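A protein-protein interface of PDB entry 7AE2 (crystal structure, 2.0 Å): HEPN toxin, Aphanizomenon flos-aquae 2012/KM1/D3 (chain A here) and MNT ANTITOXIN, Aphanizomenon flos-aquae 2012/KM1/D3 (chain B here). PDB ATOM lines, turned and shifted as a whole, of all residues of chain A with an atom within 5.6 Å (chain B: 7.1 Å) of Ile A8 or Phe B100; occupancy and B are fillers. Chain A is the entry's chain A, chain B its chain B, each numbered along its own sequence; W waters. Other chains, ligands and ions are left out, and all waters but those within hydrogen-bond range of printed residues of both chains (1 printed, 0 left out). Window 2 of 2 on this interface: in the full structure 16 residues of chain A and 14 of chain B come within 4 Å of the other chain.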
ATOM      1  N   GLU A   5      29.850   5.139  -0.544  1.00  0.00           N
ATOM      2  CA  GLU A   5      29.811   3.685  -0.475  1.00  0.00           C
ATOM      3  C   GLU A   5      30.945   3.104  -1.313  1.00  0.00           C
ATOM      4  O   GLU A   5      30.867   3.101  -2.547  1.00  0.00           O
ATOM      5  CB  GLU A   5      28.457   3.150  -0.950  1.00  0.00           C
ATOM      6  CG  GLU A   5      27.280   3.545  -0.079  1.00  0.00           C
ATOM      7  CD  GLU A   5      27.282   2.856   1.274  1.00  0.00           C
ATOM      8  OE1 GLU A   5      26.724   3.434   2.231  1.00  0.00           O
ATOM      9  OE2 GLU A   5      27.840   1.745   1.386  1.00  0.00           O
ATOM     10  N   PRO A   6      32.014   2.618  -0.679  1.00  0.00           N
ATOM     11  CA  PRO A   6      33.145   2.080  -1.452  1.00  0.00           C
ATOM     12  C   PRO A   6      32.785   0.869  -2.296  1.00  0.00           C
ATOM     13  O   PRO A   6      33.352   0.692  -3.383  1.00  0.00           O
ATOM     14  CB  PRO A   6      34.170   1.725  -0.364  1.00  0.00           C
ATOM     15  CG  PRO A   6      33.767   2.536   0.837  1.00  0.00           C
ATOM     16  CD  PRO A   6      32.277   2.610   0.767  1.00  0.00           C
ATOM     17  N   VAL A   7      31.863   0.023  -1.830  1.00  0.00           N
ATOM     18  CA  VAL A   7      31.540  -1.189  -2.577  1.00  0.00           C
ATOM     19  C   VAL A   7      30.869  -0.849  -3.905  1.00  0.00           C
ATOM     20  O   VAL A   7      31.022  -1.583  -4.890  1.00  0.00           O
ATOM     21  CB  VAL A   7      30.676  -2.133  -1.716  1.00  0.00           C
ATOM     22  CG1 VAL A   7      29.294  -1.538  -1.464  1.00  0.00           C
ATOM     23  CG2 VAL A   7      30.575  -3.510  -2.361  1.00  0.00           C
ATOM     24  N   ILE A   8      30.142   0.269  -3.971  1.00  0.00           N
ATOM     25  CA  ILE A   8      29.547   0.691  -5.236  1.00  0.00           C
ATOM     26  C   ILE A   8      30.626   1.167  -6.199  1.00  0.00           C
ATOM     27  O   ILE A   8      30.615   0.823  -7.388  1.00  0.00           O
ATOM     28  CB  ILE A   8      28.481   1.776  -4.991  1.00  0.00           C
ATOM     29  CG1 ILE A   8      27.258   1.177  -4.291  1.00  0.00           C
ATOM     30  CG2 ILE A   8      28.080   2.442  -6.301  1.00  0.00           C
ATOM     31  CD1 ILE A   8      26.498   0.164  -5.132  1.00  0.00           C
ATOM     32  N   ILE A   9      31.577   1.962  -5.704  1.00  0.00           N
ATOM     33  CA  ILE A   9      32.668   2.437  -6.548  1.00  0.00           C
ATOM     34  C   ILE A   9      33.558   1.278  -6.982  1.00  0.00           C
ATOM     35  O   ILE A   9      33.994   1.211  -8.137  1.00  0.00           O
ATOM     36  CB  ILE A   9      33.467   3.528  -5.811  1.00  0.00           C
ATOM     37  CG1 ILE A   9      32.568   4.728  -5.504  1.00  0.00           C
ATOM     38  CG2 ILE A   9      34.678   3.960  -6.629  1.00  0.00           C
ATOM     39  CD1 ILE A   9      33.277   5.857  -4.792  1.00  0.00           C
ATOM     40  N   GLU A  10      33.829   0.339  -6.071  1.00  0.00           N
ATOM     41  CA  GLU A  10      34.679  -0.800  -6.407  1.00  0.00           C
ATOM     42  C   GLU A  10      34.054  -1.656  -7.502  1.00  0.00           C
ATOM     43  O   GLU A  10      34.765  -2.190  -8.363  1.00  0.00           O
ATOM     44  CB  GLU A  10      34.953  -1.633  -5.155  1.00  0.00           C
ATOM     45  CG  GLU A  10      35.904  -0.961  -4.180  1.00  0.00           C
ATOM     46  CD  GLU A  10      35.704  -1.418  -2.749  1.00  0.00           C
ATOM     47  OE1 GLU A  10      34.858  -2.305  -2.516  1.00  0.00           O
ATOM     48  OE2 GLU A  10      36.393  -0.883  -1.854  1.00  0.00           O
ATOM     49  N   THR A  11      32.726  -1.795  -7.487  1.00  0.00           N
ATOM     50  CA  THR A  11      32.045  -2.529  -8.549  1.00  0.00           C
ATOM     51  C   THR A  11      32.286  -1.884  -9.909  1.00  0.00           C
ATOM     52  O   THR A  11      32.537  -2.579 -10.900  1.00  0.00           O
ATOM     53  CB  THR A  11      30.547  -2.612  -8.256  1.00  0.00           C
ATOM     54  OG1 THR A  11      30.335  -3.303  -7.018  1.00  0.00           O
ATOM     55  CG2 THR A  11      29.821  -3.350  -9.371  1.00  0.00           C
ATOM     56  N   ARG A  12      32.222  -0.552  -9.976  1.00  0.00           N
ATOM     57  CA  ARG A  12      32.423   0.126 -11.253  1.00  0.00           C
ATOM     58  C   ARG A  12      33.887   0.096 -11.677  1.00  0.00           C
ATOM     59  O   ARG A  12      34.187  -0.047 -12.868  1.00  0.00           O
ATOM     60  CB  ARG A  12      31.913   1.564 -11.169  1.00  0.00           C
ATOM     61  CG  ARG A  12      30.418   1.672 -10.927  1.00  0.00           C
ATOM     62  CD  ARG A  12      29.637   0.977 -12.029  1.00  0.00           C
ATOM     63  NE  ARG A  12      28.196   1.156 -11.879  1.00  0.00           N
ATOM     64  CZ  ARG A  12      27.291   0.604 -12.680  1.00  0.00           C
ATOM     65  NH1 ARG A  12      27.680  -0.164 -13.688  1.00  0.00           N
ATOM     66  NH2 ARG A  12      25.999   0.819 -12.474  1.00  0.00           N
ATOM     67  N   LEU A  13      34.813   0.238 -10.725  1.00  0.00           N
ATOM     68  CA  LEU A  13      36.228   0.108 -11.060  1.00  0.00           C
ATOM     69  C   LEU A  13      36.534  -1.285 -11.592  1.00  0.00           C
ATOM     70  O   LEU A  13      37.333  -1.441 -12.523  1.00  0.00           O
ATOM     71  CB  LEU A  13      37.096   0.409  -9.838  1.00  0.00           C
ATOM     72  CG  LEU A  13      37.276   1.866  -9.425  1.00  0.00           C
ATOM     73  CD1 LEU A  13      38.201   1.933  -8.219  1.00  0.00           C
ATOM     74  CD2 LEU A  13      37.835   2.691 -10.579  1.00  0.00           C
ATOM     75  N   ASP A  57      29.837   7.581 -13.615  1.00  0.00           N
ATOM     76  CA  ASP A  57      29.061   7.087 -12.480  1.00  0.00           C
ATOM     77  C   ASP A  57      29.856   7.188 -11.184  1.00  0.00           C
ATOM     78  O   ASP A  57      29.300   7.520 -10.130  1.00  0.00           O
ATOM     79  CB  ASP A  57      28.623   5.643 -12.731  1.00  0.00           C
ATOM     80  CG  ASP A  57      27.597   5.157 -11.720  1.00  0.00           C
ATOM     81  OD1 ASP A  57      26.885   6.002 -11.137  1.00  0.00           O
ATOM     82  OD2 ASP A  57      27.506   3.929 -11.505  1.00  0.00           O
ATOM     83  N   HIS A  61      29.113   9.843  -7.918  1.00  0.00           N
ATOM     84  CA  HIS A  61      28.909   9.295  -6.580  1.00  0.00           C
ATOM     85  C   HIS A  61      29.840   9.956  -5.572  1.00  0.00           C
ATOM     86  O   HIS A  61      29.432  10.263  -4.445  1.00  0.00           O
ATOM     87  CB  HIS A  61      29.111   7.779  -6.589  1.00  0.00           C
ATOM     88  N   PHE B  31      14.483   4.842  -5.816  1.00  0.00           N
ATOM     89  CA  PHE B  31      15.769   4.951  -5.144  1.00  0.00           C
ATOM     90  C   PHE B  31      16.631   5.947  -5.907  1.00  0.00           C
ATOM     91  O   PHE B  31      16.223   6.500  -6.933  1.00  0.00           O
ATOM     92  CB  PHE B  31      16.457   3.585  -5.023  1.00  0.00           C
ATOM     93  CG  PHE B  31      16.814   2.959  -6.345  1.00  0.00           C
ATOM     94  CD1 PHE B  31      15.879   2.226  -7.057  1.00  0.00           C
ATOM     95  CD2 PHE B  31      18.090   3.095  -6.867  1.00  0.00           C
ATOM     96  CE1 PHE B  31      16.209   1.646  -8.272  1.00  0.00           C
ATOM     97  CE2 PHE B  31      18.426   2.518  -8.078  1.00  0.00           C
ATOM     98  CZ  PHE B  31      17.485   1.793  -8.781  1.00  0.00           C
ATOM     99  N   GLY B  32      17.834   6.178  -5.393  1.00  0.00           N
ATOM    100  CA  GLY B  32      18.741   7.123  -6.009  1.00  0.00           C
ATOM    101  C   GLY B  32      18.604   8.527  -5.460  1.00  0.00           C
ATOM    102  O   GLY B  32      18.262   8.718  -4.290  1.00  0.00           O
ATOM    103  N   LYS B  95      22.980  -9.280  -6.030  1.00  0.00           N
ATOM    104  CA  LYS B  95      22.591  -9.159  -4.629  1.00  0.00           C
ATOM    105  C   LYS B  95      22.993  -7.803  -4.065  1.00  0.00           C
ATOM    106  O   LYS B  95      22.401  -7.334  -3.087  1.00  0.00           O
ATOM    107  CB  LYS B  95      23.215 -10.290  -3.804  1.00  0.00           C
ATOM    108  N   LEU B  96      23.992  -7.159  -4.672  1.00  0.00           N
ATOM    109  CA  LEU B  96      24.437  -5.853  -4.205  1.00  0.00           C
ATOM    110  C   LEU B  96      23.411  -4.772  -4.528  1.00  0.00           C
ATOM    111  O   LEU B  96      23.122  -3.919  -3.681  1.00  0.00           O
ATOM    112  CB  LEU B  96      25.799  -5.529  -4.821  1.00  0.00           C
ATOM    113  CG  LEU B  96      26.629  -4.502  -4.068  1.00  0.00           C
ATOM    114  CD1 LEU B  96      26.887  -4.964  -2.635  1.00  0.00           C
ATOM    115  CD2 LEU B  96      27.931  -4.257  -4.807  1.00  0.00           C
ATOM    116  N   ILE B  97      22.859  -4.778  -5.744  1.00  0.00           N
ATOM    117  CA  ILE B  97      21.866  -3.768  -6.103  1.00  0.00           C
ATOM    118  C   ILE B  97      20.603  -3.933  -5.263  1.00  0.00           C
ATOM    119  O   ILE B  97      20.002  -2.947  -4.820  1.00  0.00           O
ATOM    120  CB  ILE B  97      21.554  -3.830  -7.610  1.00  0.00           C
ATOM    121  N   ALA B  98      20.181  -5.176  -5.023  1.00  0.00           N
ATOM    122  CA  ALA B  98      18.979  -5.393  -4.224  1.00  0.00           C
ATOM    123  C   ALA B  98      19.163  -4.910  -2.791  1.00  0.00           C
ATOM    124  O   ALA B  98      18.197  -4.476  -2.151  1.00  0.00           O
ATOM    125  CB  ALA B  98      18.588  -6.871  -4.240  1.00  0.00           C
ATOM    126  N   HIS B  99      20.394  -4.964  -2.281  1.00  0.00           N
ATOM    127  CA  HIS B  99      20.661  -4.505  -0.922  1.00  0.00           C
ATOM    128  C   HIS B  99      20.414  -3.007  -0.785  1.00  0.00           C
ATOM    129  O   HIS B  99      19.712  -2.562   0.130  1.00  0.00           O
ATOM    130  CB  HIS B  99      22.097  -4.853  -0.531  1.00  0.00           C
ATOM    131  CG  HIS B  99      22.555  -4.189   0.728  1.00  0.00           C
ATOM    132  ND1 HIS B  99      22.157  -4.609   1.979  1.00  0.00           N
ATOM    133  CD2 HIS B  99      23.368  -3.126   0.931  1.00  0.00           C
ATOM    134  CE1 HIS B  99      22.710  -3.838   2.898  1.00  0.00           C
ATOM    135  NE2 HIS B  99      23.449  -2.929   2.288  1.00  0.00           N
ATOM    136  N   PHE B 100      20.986  -2.211  -1.692  1.00  0.00           N
ATOM    137  CA  PHE B 100      20.853  -0.762  -1.582  1.00  0.00           C
ATOM    138  C   PHE B 100      19.452  -0.291  -1.950  1.00  0.00           C
ATOM    139  O   PHE B 100      19.001   0.747  -1.455  1.00  0.00           O
ATOM    140  CB  PHE B 100      21.903  -0.071  -2.452  1.00  0.00           C
ATOM    141  CG  PHE B 100      23.312  -0.269  -1.966  1.00  0.00           C
ATOM    142  CD1 PHE B 100      23.805   0.481  -0.910  1.00  0.00           C
ATOM    143  CD2 PHE B 100      24.142  -1.206  -2.559  1.00  0.00           C
ATOM    144  CE1 PHE B 100      25.100   0.300  -0.455  1.00  0.00           C
ATOM    145  CE2 PHE B 100      25.438  -1.392  -2.109  1.00  0.00           C
ATOM    146  CZ  PHE B 100      25.916  -0.637  -1.056  1.00  0.00           C
ATOM    147  N   VAL B 101      18.750  -1.032  -2.810  1.00  0.00           N
ATOM    148  CA  VAL B 101      17.357  -0.700  -3.091  1.00  0.00           C
ATOM    149  C   VAL B 101      16.500  -0.925  -1.851  1.00  0.00           C
ATOM    150  O   VAL B 101      15.610  -0.124  -1.540  1.00  0.00           O
ATOM    151  CB  VAL B 101      16.847  -1.509  -4.300  1.00  0.00           C
ATOM    152  CG1 VAL B 101      15.336  -1.385  -4.430  1.00  0.00           C
ATOM    153  CG2 VAL B 101      17.528  -1.032  -5.575  1.00  0.00           C
ATOM    154  N   ALA B 102      16.765  -2.004  -1.110  1.00  0.00           N
ATOM    155  CA  ALA B 102      16.022  -2.260   0.119  1.00  0.00           C
ATOM    156  C   ALA B 102      16.419  -1.296   1.231  1.00  0.00           C
ATOM    157  O   ALA B 102      15.588  -0.955   2.079  1.00  0.00           O
ATOM    158  CB  ALA B 102      16.233  -3.704   0.571  1.00  0.00           C
ATOM    159  N   ARG B 103      17.674  -0.841   1.235  1.00  0.00           N
ATOM    160  CA  ARG B 103      18.165   0.015   2.309  1.00  0.00           C
ATOM    161  C   ARG B 103      17.708   1.460   2.136  1.00  0.00           C
ATOM    162  O   ARG B 103      17.238   2.088   3.092  1.00  0.00           O
ATOM    163  CB  ARG B 103      19.692  -0.049   2.377  1.00  0.00           C
ATOM    164  CG  ARG B 103      20.274   0.492   3.672  1.00  0.00           C
ATOM    165  CD  ARG B 103      21.781   0.673   3.579  1.00  0.00           C
ATOM    166  NE  ARG B 103      22.141   1.757   2.672  1.00  0.00           N
ATOM    167  CZ  ARG B 103      23.387   2.173   2.464  1.00  0.00           C
ATOM    168  NH1 ARG B 103      24.395   1.593   3.100  1.00  0.00           N
ATOM    169  NH2 ARG B 103      23.623   3.169   1.622  1.00  0.00           N
ATOM    170  N   ASP B 104      17.847   2.008   0.930  1.00  0.00           N
ATOM    171  CA  ASP B 104      17.578   3.419   0.686  1.00  0.00           C
ATOM    172  C   ASP B 104      16.334   3.666  -0.154  1.00  0.00           C
ATOM    173  O   ASP B 104      15.968   4.827  -0.364  1.00  0.00           O
ATOM    174  CB  ASP B 104      18.787   4.079   0.005  1.00  0.00           C
ATOM    175  CG  ASP B 104      20.041   4.049   0.867  1.00  0.00           C
ATOM    176  OD1 ASP B 104      19.920   4.087   2.111  1.00  0.00           O
ATOM    177  OD2 ASP B 104      21.152   3.998   0.295  1.00  0.00           O
ATOM    178  N   GLY B 105      15.673   2.619  -0.640  1.00  0.00           N
ATOM    179  CA  GLY B 105      14.542   2.812  -1.526  1.00  0.00           C
ATOM    180  C   GLY B 105      13.280   3.228  -0.792  1.00  0.00           C
ATOM    181  O   GLY B 105      13.060   2.894   0.371  1.00  0.00           O
ATOM    182  N   PHE B 119      10.578  -8.097   1.011  1.00  0.00           N
ATOM    183  CA  PHE B 119      11.720  -7.888   0.127  1.00  0.00           C
ATOM    184  C   PHE B 119      12.962  -7.497   0.920  1.00  0.00           C
ATOM    185  O   PHE B 119      14.055  -8.019   0.676  1.00  0.00           O
ATOM    186  CB  PHE B 119      11.381  -6.825  -0.918  1.00  0.00           C
ATOM    187  CG  PHE B 119      12.570  -6.322  -1.685  1.00  0.00           C
ATOM    188  CD1 PHE B 119      13.208  -7.129  -2.610  1.00  0.00           C
ATOM    189  CD2 PHE B 119      13.043  -5.036  -1.485  1.00  0.00           C
ATOM    190  CE1 PHE B 119      14.301  -6.665  -3.318  1.00  0.00           C
ATOM    191  CE2 PHE B 119      14.133  -4.566  -2.190  1.00  0.00           C
ATOM    192  CZ  PHE B 119      14.764  -5.381  -3.108  1.00  0.00           C
ATOM    193  N   VAL B 123      16.682  -9.630   1.030  1.00  0.00           N
ATOM    194  CA  VAL B 123      17.838  -9.191   0.255  1.00  0.00           C
ATOM    195  C   VAL B 123      18.823  -8.347   1.051  1.00  0.00           C
ATOM    196  O   VAL B 123      19.919  -8.069   0.541  1.00  0.00           O
ATOM    197  CB  VAL B 123      17.407  -8.427  -1.016  1.00  0.00           C
ATOM    198  CG1 VAL B 123      16.366  -9.223  -1.794  1.00  0.00           C
ATOM    199  CG2 VAL B 123      16.883  -7.050  -0.655  1.00  0.00           C
ATOM    200  N   LEU B 124      18.490  -7.923   2.268  1.00  0.00           N
ATOM    201  CA  LEU B 124      19.400  -7.074   3.030  1.00  0.00           C
ATOM    202  C   LEU B 124      20.638  -7.854   3.458  1.00  0.00           C
ATOM    203  O   LEU B 124      20.536  -8.952   4.012  1.00  0.00           O
ATOM    204  CB  LEU B 124      18.693  -6.491   4.253  1.00  0.00           C
ATOM    205  CG  LEU B 124      17.952  -5.170   4.028  1.00  0.00           C
ATOM    206  CD1 LEU B 124      17.232  -4.731   5.296  1.00  0.00           C
ATOM    207  CD2 LEU B 124      18.919  -4.094   3.558  1.00  0.00           C
ATOM    208  N   LEU B 125      21.808  -7.276   3.203  1.00  0.00           N
ATOM    209  CA  LEU B 125      23.085  -7.881   3.546  1.00  0.00           C
ATOM    210  C   LEU B 125      23.605  -7.318   4.862  1.00  0.00           C
ATOM    211  O   LEU B 125      23.343  -6.165   5.212  1.00  0.00           O
ATOM    212  CB  LEU B 125      24.121  -7.638   2.444  1.00  0.00           C
ATOM    213  CG  LEU B 125      23.843  -8.234   1.064  1.00  0.00           C
ATOM    214  CD1 LEU B 125      24.912  -7.794   0.080  1.00  0.00           C
ATOM    215  CD2 LEU B 125      23.776  -9.751   1.144  1.00  0.00           C
ATOM    216  N   ILE B 130      29.021  -7.504   3.219  1.00  0.00           N
ATOM    217  CA  ILE B 130      29.491  -6.449   2.328  1.00  0.00           C
ATOM    218  C   ILE B 130      31.009  -6.334   2.390  1.00  0.00           C
ATOM    219  O   ILE B 130      31.668  -6.090   1.371  1.00  0.00           O
ATOM    220  CB  ILE B 130      28.805  -5.115   2.673  1.00  0.00           C
ATOM    221  CG1 ILE B 130      27.285  -5.261   2.590  1.00  0.00           C
ATOM    222  CG2 ILE B 130      29.281  -4.010   1.740  1.00  0.00           C
ATOM    223  CD1 ILE B 130      26.537  -4.002   2.961  1.00  0.00           C
ATOM    224  N   GLU B 134      33.622  -6.453  -0.633  1.00  0.00           N
ATOM    225  CA  GLU B 134      34.639  -5.427  -0.850  1.00  0.00           C
ATOM    226  C   GLU B 134      36.025  -6.040  -0.997  1.00  0.00           C
ATOM    227  O   GLU B 134      36.812  -5.610  -1.848  1.00  0.00           O
ATOM    228  CB  GLU B 134      34.625  -4.417   0.299  1.00  0.00           C
ATOM    229  CG  GLU B 134      33.383  -3.544   0.352  1.00  0.00           C
ATOM    230  CD  GLU B 134      33.420  -2.543   1.491  1.00  0.00           C
ATOM    231  OE1 GLU B 134      34.352  -2.619   2.319  1.00  0.00           O
ATOM    232  OE2 GLU B 134      32.519  -1.682   1.559  1.00  0.00           O
ATOM    233  N   LYS B 137      36.457  -7.590  -4.535  1.00  0.00           N
ATOM    234  CA  LYS B 137      36.593  -6.604  -5.599  1.00  0.00           C
ATOM    235  C   LYS B 137      37.895  -5.823  -5.479  1.00  0.00           C
ATOM    236  O   LYS B 137      38.506  -5.483  -6.498  1.00  0.00           O
ATOM    237  CB  LYS B 137      35.386  -5.669  -5.601  1.00  0.00           C
ATOM    238  CG  LYS B 137      34.070  -6.400  -5.829  1.00  0.00           C
ATOM    239  CD  LYS B 137      32.929  -5.437  -6.075  1.00  0.00           C
ATOM    240  CE  LYS B 137      31.647  -6.183  -6.406  1.00  0.00           C
ATOM    241  NZ  LYS B 137      31.817  -7.138  -7.541  1.00  0.00           N
HETATM  242  O   HOH W   1      36.307  -1.091   0.707  1.00  0.00           O
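The side-chain carboxylate (OE1) of Glu A5 lies within salt-bridge range of the guanidinium group (NH1) of Arg B103 (3.1 Å).
The backbone carbonyl oxygen of Val A7 sits at hydrogen-bond distance from the side-chain hydroxyl of Thr A11.
NH2 of Arg B103 lies within salt-bridge range of OD2 of Asp B104, 2.9 Å away.
Glu A5 touches Phe B100.
CG2 of Val A7 touches CD2 of Leu B96, 3.7 Å away.
CZ of Phe B100 touches CG1 of Val A7, at 3.5 Å.
CB of Val A7 touches CG of Glu B134, at 3.7 Å.
CD1 of Ile A8 touches CE2 of Phe B100, at 3.6 Å.
Glu A10 touches Glu B134 (OE1 to CG, 3.5 Å).
CD2 of Leu B96 touches OG1 of Thr A11 (3.4 Å).
Lys B137 touches Thr A11.
Printed residues of chain B within 4 Å of Val A7: Leu B96, Phe B100 and Glu B134.
Ile A8 touches just one residue of chain B: Phe B100 (3.6 Å).
Printed residues of chain B within 4 Å of Glu A10: Glu B134.
Printed residues of chain B within 4 Å of Thr A11: Leu B96 (3.4 Å) and Lys B137 (3.2 Å).
Of the printed residues of chain A, Leu B96 touches Val A7 and Thr A11.
Phe B100 touches just these residues of chain A: Glu A5, Val A7 and Ile A8.
Of the printed residues of chain A, Glu B134 touches Val A7 and Glu A10.
The nearest residue of chain B that does not touch Ile A8 is Leu B96 (4.7 Å).
Printed residues of chain A that touch a printed residue of chain B: Glu A5, Val A7, Ile A8, Glu A10 and Thr A11.
Printed residues of chain B that touch a printed residue of chain A: Leu B96, Phe B100, Arg B103, Glu B134 and Lys B137.
Hydrophobic or aromatic side chains of chain B within 4 Å of the printed part of chain A: Leu B96 and Phe B100.
Among the printed residues, Asp or Glu carboxylates within 4 Å of a Lys or Arg side-chain nitrogen of the other chain: Glu A5 with Arg B103 (3.1 Å).
Water W1 bridges OE2 of Glu A10 (2.6 Å) and OE1 of Glu B134 (3.0 Å).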
